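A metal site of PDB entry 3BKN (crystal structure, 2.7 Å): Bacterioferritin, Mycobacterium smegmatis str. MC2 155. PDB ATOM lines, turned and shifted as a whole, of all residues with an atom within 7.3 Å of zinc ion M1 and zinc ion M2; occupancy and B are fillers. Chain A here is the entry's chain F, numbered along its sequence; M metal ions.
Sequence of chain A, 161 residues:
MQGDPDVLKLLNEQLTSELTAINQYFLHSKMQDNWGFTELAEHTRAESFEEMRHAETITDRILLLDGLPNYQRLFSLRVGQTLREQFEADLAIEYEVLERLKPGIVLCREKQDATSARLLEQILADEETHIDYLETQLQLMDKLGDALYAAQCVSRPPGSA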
ATOM      1  N   GLN A  14      20.991 -11.048 -22.351  1.00  0.00           N
ATOM      2  CA  GLN A  14      20.426 -11.613 -21.122  1.00  0.00           C
ATOM      3  C   GLN A  14      21.349 -12.667 -20.506  1.00  0.00           C
ATOM      4  O   GLN A  14      21.538 -12.697 -19.274  1.00  0.00           O
ATOM      5  CB  GLN A  14      19.072 -12.216 -21.392  1.00  0.00           C
ATOM      6  CG  GLN A  14      18.327 -12.592 -20.172  1.00  0.00           C
ATOM      7  CD  GLN A  14      18.287 -11.517 -19.112  1.00  0.00           C
ATOM      8  OE1 GLN A  14      18.427 -10.347 -19.390  1.00  0.00           O
ATOM      9  NE2 GLN A  14      18.096 -11.935 -17.872  1.00  0.00           N
ATOM     10  N   SER A  17      23.953 -11.070 -18.604  1.00  0.00           N
ATOM     11  CA  SER A  17      23.407 -10.592 -17.323  1.00  0.00           C
ATOM     12  C   SER A  17      23.298 -11.691 -16.253  1.00  0.00           C
ATOM     13  O   SER A  17      23.662 -11.458 -15.123  1.00  0.00           O
ATOM     14  CB  SER A  17      22.082  -9.886 -17.528  1.00  0.00           C
ATOM     15  OG  SER A  17      22.190  -8.562 -17.017  1.00  0.00           O
ATOM     16  N   GLU A  18      22.830 -12.878 -16.646  1.00  0.00           N
ATOM     17  CA  GLU A  18      22.763 -14.013 -15.719  1.00  0.00           C
ATOM     18  C   GLU A  18      24.152 -14.446 -15.274  1.00  0.00           C
ATOM     19  O   GLU A  18      24.374 -14.716 -14.105  1.00  0.00           O
ATOM     20  CB  GLU A  18      22.048 -15.242 -16.291  1.00  0.00           C
ATOM     21  CG  GLU A  18      20.781 -14.980 -17.039  1.00  0.00           C
ATOM     22  CD  GLU A  18      19.588 -14.621 -16.165  1.00  0.00           C
ATOM     23  OE1 GLU A  18      19.544 -14.927 -14.940  1.00  0.00           O
ATOM     24  OE2 GLU A  18      18.653 -14.047 -16.756  1.00  0.00           O
ATOM     25  N   ALA A  21      25.157 -12.130 -12.722  1.00  0.00           N
ATOM     26  CA  ALA A  21      24.368 -12.329 -11.534  1.00  0.00           C
ATOM     27  C   ALA A  21      24.835 -13.567 -10.776  1.00  0.00           C
ATOM     28  O   ALA A  21      24.928 -13.497  -9.556  1.00  0.00           O
ATOM     29  CB  ALA A  21      22.905 -12.433 -11.859  1.00  0.00           C
ATOM     30  N   TYR A  25      25.916 -12.757  -6.907  1.00  0.00           N
ATOM     31  CA  TYR A  25      25.164 -13.418  -5.866  1.00  0.00           C
ATOM     32  C   TYR A  25      26.031 -14.458  -5.132  1.00  0.00           C
ATOM     33  O   TYR A  25      26.069 -14.489  -3.922  1.00  0.00           O
ATOM     34  CB  TYR A  25      23.994 -14.145  -6.513  1.00  0.00           C
ATOM     35  CG  TYR A  25      22.769 -13.299  -6.791  1.00  0.00           C
ATOM     36  CD1 TYR A  25      21.980 -12.794  -5.730  1.00  0.00           C
ATOM     37  CD2 TYR A  25      22.368 -13.022  -8.097  1.00  0.00           C
ATOM     38  CE1 TYR A  25      20.836 -12.039  -5.983  1.00  0.00           C
ATOM     39  CE2 TYR A  25      21.226 -12.273  -8.358  1.00  0.00           C
ATOM     40  CZ  TYR A  25      20.471 -11.790  -7.297  1.00  0.00           C
ATOM     41  OH  TYR A  25      19.342 -11.061  -7.551  1.00  0.00           O
ATOM     42  N   GLU A  47      19.555 -17.716  -4.462  1.00  0.00           N
ATOM     43  CA  GLU A  47      19.335 -16.825  -5.576  1.00  0.00           C
ATOM     44  C   GLU A  47      20.421 -17.008  -6.639  1.00  0.00           C
ATOM     45  O   GLU A  47      20.177 -16.911  -7.831  1.00  0.00           O
ATOM     46  CB  GLU A  47      19.172 -15.368  -5.103  1.00  0.00           C
ATOM     47  CG  GLU A  47      18.044 -15.144  -4.081  1.00  0.00           C
ATOM     48  CD  GLU A  47      16.648 -15.043  -4.733  1.00  0.00           C
ATOM     49  OE1 GLU A  47      16.202 -16.022  -5.413  1.00  0.00           O
ATOM     50  OE2 GLU A  47      15.977 -13.976  -4.551  1.00  0.00           O
ATOM     51  N   GLU A  50      19.465 -19.950  -8.792  1.00  0.00           N
ATOM     52  CA  GLU A  50      18.381 -19.611  -9.635  1.00  0.00           C
ATOM     53  C   GLU A  50      18.949 -18.922 -10.883  1.00  0.00           C
ATOM     54  O   GLU A  50      18.465 -19.176 -11.999  1.00  0.00           O
ATOM     55  CB  GLU A  50      17.372 -18.763  -8.882  1.00  0.00           C
ATOM     56  CG  GLU A  50      15.967 -19.205  -9.187  1.00  0.00           C
ATOM     57  CD  GLU A  50      14.980 -18.490  -8.363  1.00  0.00           C
ATOM     58  OE1 GLU A  50      15.096 -18.528  -7.104  1.00  0.00           O
ATOM     59  OE2 GLU A  50      14.084 -17.877  -8.989  1.00  0.00           O
ATOM     60  N   GLU A  51      19.988 -18.106 -10.725  1.00  0.00           N
ATOM     61  CA  GLU A  51      20.604 -17.479 -11.862  1.00  0.00           C
ATOM     62  C   GLU A  51      21.321 -18.520 -12.738  1.00  0.00           C
ATOM     63  O   GLU A  51      21.280 -18.458 -13.973  1.00  0.00           O
ATOM     64  CB  GLU A  51      21.560 -16.398 -11.414  1.00  0.00           C
ATOM     65  CG  GLU A  51      20.879 -15.360 -10.578  1.00  0.00           C
ATOM     66  CD  GLU A  51      19.776 -14.640 -11.310  1.00  0.00           C
ATOM     67  OE1 GLU A  51      19.905 -14.437 -12.525  1.00  0.00           O
ATOM     68  OE2 GLU A  51      18.779 -14.253 -10.671  1.00  0.00           O
ATOM     69  N   MET A  52      21.962 -19.487 -12.088  1.00  0.00           N
ATOM     70  CA  MET A  52      22.521 -20.598 -12.830  1.00  0.00           C
ATOM     71  C   MET A  52      21.461 -21.276 -13.696  1.00  0.00           C
ATOM     72  O   MET A  52      21.685 -21.531 -14.866  1.00  0.00           O
ATOM     73  CB  MET A  52      23.215 -21.578 -11.911  1.00  0.00           C
ATOM     74  CG  MET A  52      24.503 -21.041 -11.334  1.00  0.00           C
ATOM     75  SD  MET A  52      25.127 -22.133 -10.021  1.00  0.00           S
ATOM     76  CE  MET A  52      25.734 -20.907  -8.851  1.00  0.00           C
ATOM     77  N   ARG A  53      20.285 -21.529 -13.139  1.00  0.00           N
ATOM     78  CA  ARG A  53      19.218 -22.070 -13.946  1.00  0.00           C
ATOM     79  C   ARG A  53      18.824 -21.192 -15.128  1.00  0.00           C
ATOM     80  O   ARG A  53      18.613 -21.729 -16.217  1.00  0.00           O
ATOM     81  CB  ARG A  53      17.985 -22.419 -13.120  1.00  0.00           C
ATOM     82  CG  ARG A  53      17.902 -23.899 -12.754  1.00  0.00           C
ATOM     83  CD  ARG A  53      16.888 -24.196 -11.607  1.00  0.00           C
ATOM     84  NE  ARG A  53      17.572 -24.182 -10.308  1.00  0.00           N
ATOM     85  CZ  ARG A  53      17.068 -23.633  -9.215  1.00  0.00           C
ATOM     86  NH1 ARG A  53      15.884 -23.037  -9.262  1.00  0.00           N
ATOM     87  NH2 ARG A  53      17.767 -23.663  -8.085  1.00  0.00           N
ATOM     88  N   HIS A  54      18.713 -19.871 -14.924  1.00  0.00           N
ATOM     89  CA  HIS A  54      18.396 -18.961 -16.023  1.00  0.00           C
ATOM     90  C   HIS A  54      19.461 -18.978 -17.118  1.00  0.00           C
ATOM     91  O   HIS A  54      19.138 -18.983 -18.288  1.00  0.00           O
ATOM     92  CB  HIS A  54      18.217 -17.511 -15.574  1.00  0.00           C
ATOM     93  CG  HIS A  54      17.036 -17.302 -14.696  1.00  0.00           C
ATOM     94  ND1 HIS A  54      16.848 -16.135 -13.975  1.00  0.00           N
ATOM     95  CD2 HIS A  54      15.981 -18.098 -14.395  1.00  0.00           C
ATOM     96  CE1 HIS A  54      15.732 -16.228 -13.271  1.00  0.00           C
ATOM     97  NE2 HIS A  54      15.186 -17.416 -13.514  1.00  0.00           N
ATOM     98  N   ALA A  55      20.729 -18.970 -16.737  1.00  0.00           N
ATOM     99  CA  ALA A  55      21.811 -19.088 -17.671  1.00  0.00           C
ATOM    100  C   ALA A  55      21.641 -20.367 -18.491  1.00  0.00           C
ATOM    101  O   ALA A  55      21.795 -20.317 -19.722  1.00  0.00           O
ATOM    102  CB  ALA A  55      23.162 -19.082 -16.947  1.00  0.00           C
ATOM    103  N   ILE A  58      18.588 -20.188 -21.038  1.00  0.00           N
ATOM    104  CA  ILE A  58      18.904 -19.337 -22.162  1.00  0.00           C
ATOM    105  C   ILE A  58      19.893 -20.063 -23.080  1.00  0.00           C
ATOM    106  O   ILE A  58      19.709 -20.078 -24.288  1.00  0.00           O
ATOM    107  CB  ILE A  58      19.428 -17.927 -21.751  1.00  0.00           C
ATOM    108  CG1 ILE A  58      18.290 -17.144 -21.119  1.00  0.00           C
ATOM    109  CG2 ILE A  58      19.977 -17.136 -22.967  1.00  0.00           C
ATOM    110  CD1 ILE A  58      18.711 -15.980 -20.383  1.00  0.00           C
ATOM    111  N   ASP A  90      22.733  -5.987  -5.830  1.00  0.00           N
ATOM    112  CA  ASP A  90      21.958  -7.022  -6.491  1.00  0.00           C
ATOM    113  C   ASP A  90      20.656  -6.477  -7.043  1.00  0.00           C
ATOM    114  O   ASP A  90      20.163  -6.943  -8.071  1.00  0.00           O
ATOM    115  CB  ASP A  90      21.724  -8.207  -5.551  1.00  0.00           C
ATOM    116  CG  ASP A  90      23.034  -8.963  -5.247  1.00  0.00           C
ATOM    117  OD1 ASP A  90      23.862  -9.135  -6.198  1.00  0.00           O
ATOM    118  OD2 ASP A  90      23.257  -9.378  -4.067  1.00  0.00           O
ATOM    119  N   ILE A  93      21.353  -4.852 -10.546  1.00  0.00           N
ATOM    120  CA  ILE A  93      21.395  -5.695 -11.749  1.00  0.00           C
ATOM    121  C   ILE A  93      20.078  -6.348 -12.100  1.00  0.00           C
ATOM    122  O   ILE A  93      19.837  -6.613 -13.280  1.00  0.00           O
ATOM    123  CB  ILE A  93      22.668  -6.585 -11.916  1.00  0.00           C
ATOM    124  CG1 ILE A  93      22.635  -7.867 -11.176  1.00  0.00           C
ATOM    125  CG2 ILE A  93      23.962  -5.861 -11.458  1.00  0.00           C
ATOM    126  CD1 ILE A  93      23.963  -8.530 -11.495  1.00  0.00           C
ATOM    127  N   GLU A  94      19.197  -6.528 -11.105  1.00  0.00           N
ATOM    128  CA  GLU A  94      17.842  -6.963 -11.403  1.00  0.00           C
ATOM    129  C   GLU A  94      17.084  -5.871 -12.179  1.00  0.00           C
ATOM    130  O   GLU A  94      16.352  -6.162 -13.130  1.00  0.00           O
ATOM    131  CB  GLU A  94      17.082  -7.403 -10.150  1.00  0.00           C
ATOM    132  CG  GLU A  94      17.683  -8.590  -9.387  1.00  0.00           C
ATOM    133  CD  GLU A  94      17.602  -9.880 -10.178  1.00  0.00           C
ATOM    134  OE1 GLU A  94      17.364  -9.802 -11.393  1.00  0.00           O
ATOM    135  OE2 GLU A  94      17.775 -10.987  -9.604  1.00  0.00           O
ATOM    136  N   VAL A  97      17.915  -5.996 -15.700  1.00  0.00           N
ATOM    137  CA  VAL A  97      17.211  -7.082 -16.382  1.00  0.00           C
ATOM    138  C   VAL A  97      15.837  -6.585 -16.861  1.00  0.00           C
ATOM    139  O   VAL A  97      15.484  -6.716 -18.042  1.00  0.00           O
ATOM    140  CB  VAL A  97      17.105  -8.365 -15.542  1.00  0.00           C
ATOM    141  CG1 VAL A  97      16.096  -9.355 -16.177  1.00  0.00           C
ATOM    142  CG2 VAL A  97      18.470  -9.005 -15.418  1.00  0.00           C
ATOM    143  N   ILE A 123      11.636 -15.731 -17.075  1.00  0.00           N
ATOM    144  CA  ILE A 123      12.743 -15.091 -16.388  1.00  0.00           C
ATOM    145  C   ILE A 123      12.319 -13.780 -15.758  1.00  0.00           C
ATOM    146  O   ILE A 123      12.551 -13.581 -14.580  1.00  0.00           O
ATOM    147  CB  ILE A 123      13.989 -14.994 -17.258  1.00  0.00           C
ATOM    148  CG1 ILE A 123      14.678 -16.356 -17.217  1.00  0.00           C
ATOM    149  CG2 ILE A 123      14.954 -13.962 -16.744  1.00  0.00           C
ATOM    150  CD1 ILE A 123      15.237 -16.707 -18.517  1.00  0.00           C
ATOM    151  N   LEU A 124      11.648 -12.926 -16.533  1.00  0.00           N
ATOM    152  CA  LEU A 124      11.202 -11.634 -16.036  1.00  0.00           C
ATOM    153  C   LEU A 124      10.441 -11.778 -14.717  1.00  0.00           C
ATOM    154  O   LEU A 124      10.762 -11.076 -13.733  1.00  0.00           O
ATOM    155  CB  LEU A 124      10.368 -10.907 -17.085  1.00  0.00           C
ATOM    156  CG  LEU A 124       9.904  -9.501 -16.669  1.00  0.00           C
ATOM    157  CD1 LEU A 124      11.113  -8.631 -16.552  1.00  0.00           C
ATOM    158  CD2 LEU A 124       8.919  -8.907 -17.650  1.00  0.00           C
ATOM    159  N   ASP A 126      10.524 -14.249 -12.539  1.00  0.00           N
ATOM    160  CA  ASP A 126      11.489 -14.613 -11.511  1.00  0.00           C
ATOM    161  C   ASP A 126      12.268 -13.399 -11.027  1.00  0.00           C
ATOM    162  O   ASP A 126      12.378 -13.214  -9.841  1.00  0.00           O
ATOM    163  CB  ASP A 126      12.485 -15.678 -11.955  1.00  0.00           C
ATOM    164  CG  ASP A 126      11.866 -17.076 -12.087  1.00  0.00           C
ATOM    165  OD1 ASP A 126      10.767 -17.311 -11.514  1.00  0.00           O
ATOM    166  OD2 ASP A 126      12.503 -17.935 -12.777  1.00  0.00           O
ATOM    167  N   GLU A 127      12.796 -12.582 -11.920  1.00  0.00           N
ATOM    168  CA  GLU A 127      13.555 -11.394 -11.499  1.00  0.00           C
ATOM    169  C   GLU A 127      12.673 -10.340 -10.788  1.00  0.00           C
ATOM    170  O   GLU A 127      13.167  -9.626  -9.915  1.00  0.00           O
ATOM    171  CB  GLU A 127      14.407 -10.778 -12.637  1.00  0.00           C
ATOM    172  CG  GLU A 127      15.128 -11.815 -13.555  1.00  0.00           C
ATOM    173  CD  GLU A 127      16.424 -12.415 -12.975  1.00  0.00           C
ATOM    174  OE1 GLU A 127      16.518 -12.786 -11.795  1.00  0.00           O
ATOM    175  OE2 GLU A 127      17.395 -12.550 -13.714  1.00  0.00           O
ATOM    176  N   GLU A 128      11.384 -10.240 -11.129  1.00  0.00           N
ATOM    177  CA  GLU A 128      10.489  -9.311 -10.412  1.00  0.00           C
ATOM    178  C   GLU A 128      10.353  -9.786  -8.960  1.00  0.00           C
ATOM    179  O   GLU A 128      10.350  -8.978  -8.044  1.00  0.00           O
ATOM    180  CB  GLU A 128       9.124  -9.131 -11.080  1.00  0.00           C
ATOM    181  CG  GLU A 128       9.145  -8.328 -12.403  1.00  0.00           C
ATOM    182  CD  GLU A 128       7.737  -8.045 -13.018  1.00  0.00           C
ATOM    183  OE1 GLU A 128       6.816  -7.635 -12.276  1.00  0.00           O
ATOM    184  OE2 GLU A 128       7.548  -8.209 -14.252  1.00  0.00           O
ATOM    185  N   THR A 129      10.263 -11.099  -8.752  1.00  0.00           N
ATOM    186  CA  THR A 129      10.285 -11.650  -7.422  1.00  0.00           C
ATOM    187  C   THR A 129      11.556 -11.297  -6.627  1.00  0.00           C
ATOM    188  O   THR A 129      11.448 -10.929  -5.468  1.00  0.00           O
ATOM    189  CB  THR A 129      10.057 -13.194  -7.478  1.00  0.00           C
ATOM    190  OG1 THR A 129       8.748 -13.431  -7.999  1.00  0.00           O
ATOM    191  CG2 THR A 129      10.145 -13.868  -6.115  1.00  0.00           C
ATOM    192  N   HIS A 130      12.733 -11.420  -7.237  1.00  0.00           N
ATOM    193  CA  HIS A 130      13.971 -11.040  -6.548  1.00  0.00           C
ATOM    194  C   HIS A 130      13.950  -9.579  -6.162  1.00  0.00           C
ATOM    195  O   HIS A 130      14.247  -9.243  -5.025  1.00  0.00           O
ATOM    196  CB  HIS A 130      15.196 -11.304  -7.386  1.00  0.00           C
ATOM    197  CG  HIS A 130      15.427 -12.740  -7.678  1.00  0.00           C
ATOM    198  ND1 HIS A 130      16.487 -13.176  -8.446  1.00  0.00           N
ATOM    199  CD2 HIS A 130      14.711 -13.836  -7.361  1.00  0.00           C
ATOM    200  CE1 HIS A 130      16.443 -14.490  -8.549  1.00  0.00           C
ATOM    201  NE2 HIS A 130      15.357 -14.923  -7.920  1.00  0.00           N
ATOM    202  N   ILE A 131      13.594  -8.728  -7.107  1.00  0.00           N
ATOM    203  CA  ILE A 131      13.419  -7.293  -6.853  1.00  0.00           C
ATOM    204  C   ILE A 131      12.514  -7.074  -5.646  1.00  0.00           C
ATOM    205  O   ILE A 131      12.834  -6.304  -4.753  1.00  0.00           O
ATOM    206  CB  ILE A 131      12.920  -6.531  -8.123  1.00  0.00           C
ATOM    207  CG1 ILE A 131      14.025  -6.502  -9.180  1.00  0.00           C
ATOM    208  CG2 ILE A 131      12.473  -5.122  -7.769  1.00  0.00           C
ATOM    209  CD1 ILE A 131      13.774  -5.532 -10.401  1.00  0.00           C
ATOM    210  N   LEU A 134      14.391  -8.042  -2.457  1.00  0.00           N
ATOM    211  CA  LEU A 134      15.494  -7.143  -2.168  1.00  0.00           C
ATOM    212  C   LEU A 134      15.007  -5.786  -1.667  1.00  0.00           C
ATOM    213  O   LEU A 134      15.518  -5.285  -0.661  1.00  0.00           O
ATOM    214  CB  LEU A 134      16.397  -7.008  -3.381  1.00  0.00           C
ATOM    215  CG  LEU A 134      17.259  -8.203  -3.819  1.00  0.00           C
ATOM    216  CD1 LEU A 134      17.626  -7.922  -5.259  1.00  0.00           C
ATOM    217  CD2 LEU A 134      18.509  -8.389  -2.941  1.00  0.00           C
HETATM  218 ZN    ZN M   1      17.362 -12.636 -10.306  1.00  0.00          ZN
HETATM  219 ZN    ZN M   2      18.104 -14.470 -13.812  1.00  0.00          ZN
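OE2 of Glu 94 lies close to OH of Tyr 25, 2.6 Å away. The side-chain amide nitrogen of Gln 14 lies within hydrogen-bond range of the side-chain carboxylate of Glu 18 (2.5 Å). OD2 of Asp 126 lies within hydrogen-bond range of NE2 of His 54 (2.8 Å). The side-chain carboxylate (OE2) of Glu 50 sits at hydrogen-bond distance from a ring nitrogen (NE2) of His 130 (3.4 Å). The side-chain carboxylate of Glu 47 is in hydrogen-bond range of a ring nitrogen (NE2) of His 130 (2.9 Å).
Merely in contact with zinc ion M1: Tyr 25. Of the 26 residues printed, 5 come within 4 Å of zinc ion M1. The nearest printed residue that does not touch zinc ion M1 is His 54 (4.9 Å).
Within 4 Å of zinc ion M2: Glu 18, Glu 51, His 54 and Glu 127. The nearest printed residue that does not touch zinc ion M2 is Ile 123 (4.3 Å).
OE1 of Glu 127 binds zinc ion M1. Zinc ion M1 is bound by the side-chain carboxylate (OE2) of Glu 94 (1.8 Å). A ring nitrogen (ND1) of His 130 is bound to zinc ion M1 (2.1 Å). Zinc ion M1 is bound by OE2 of Glu 51 (2.2 Å). Zinc ion M1 has four donor atoms within binding distance.
Zinc ion M2 is bound by OE1 of Glu 18 (1.9 Å), OE2 of Glu 127 (2.0 Å), ND1 of His 54 (2.1 Å) and OE1 of Glu 51 (2.2 Å). Zinc ion M2 has four donor atoms within binding distance.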
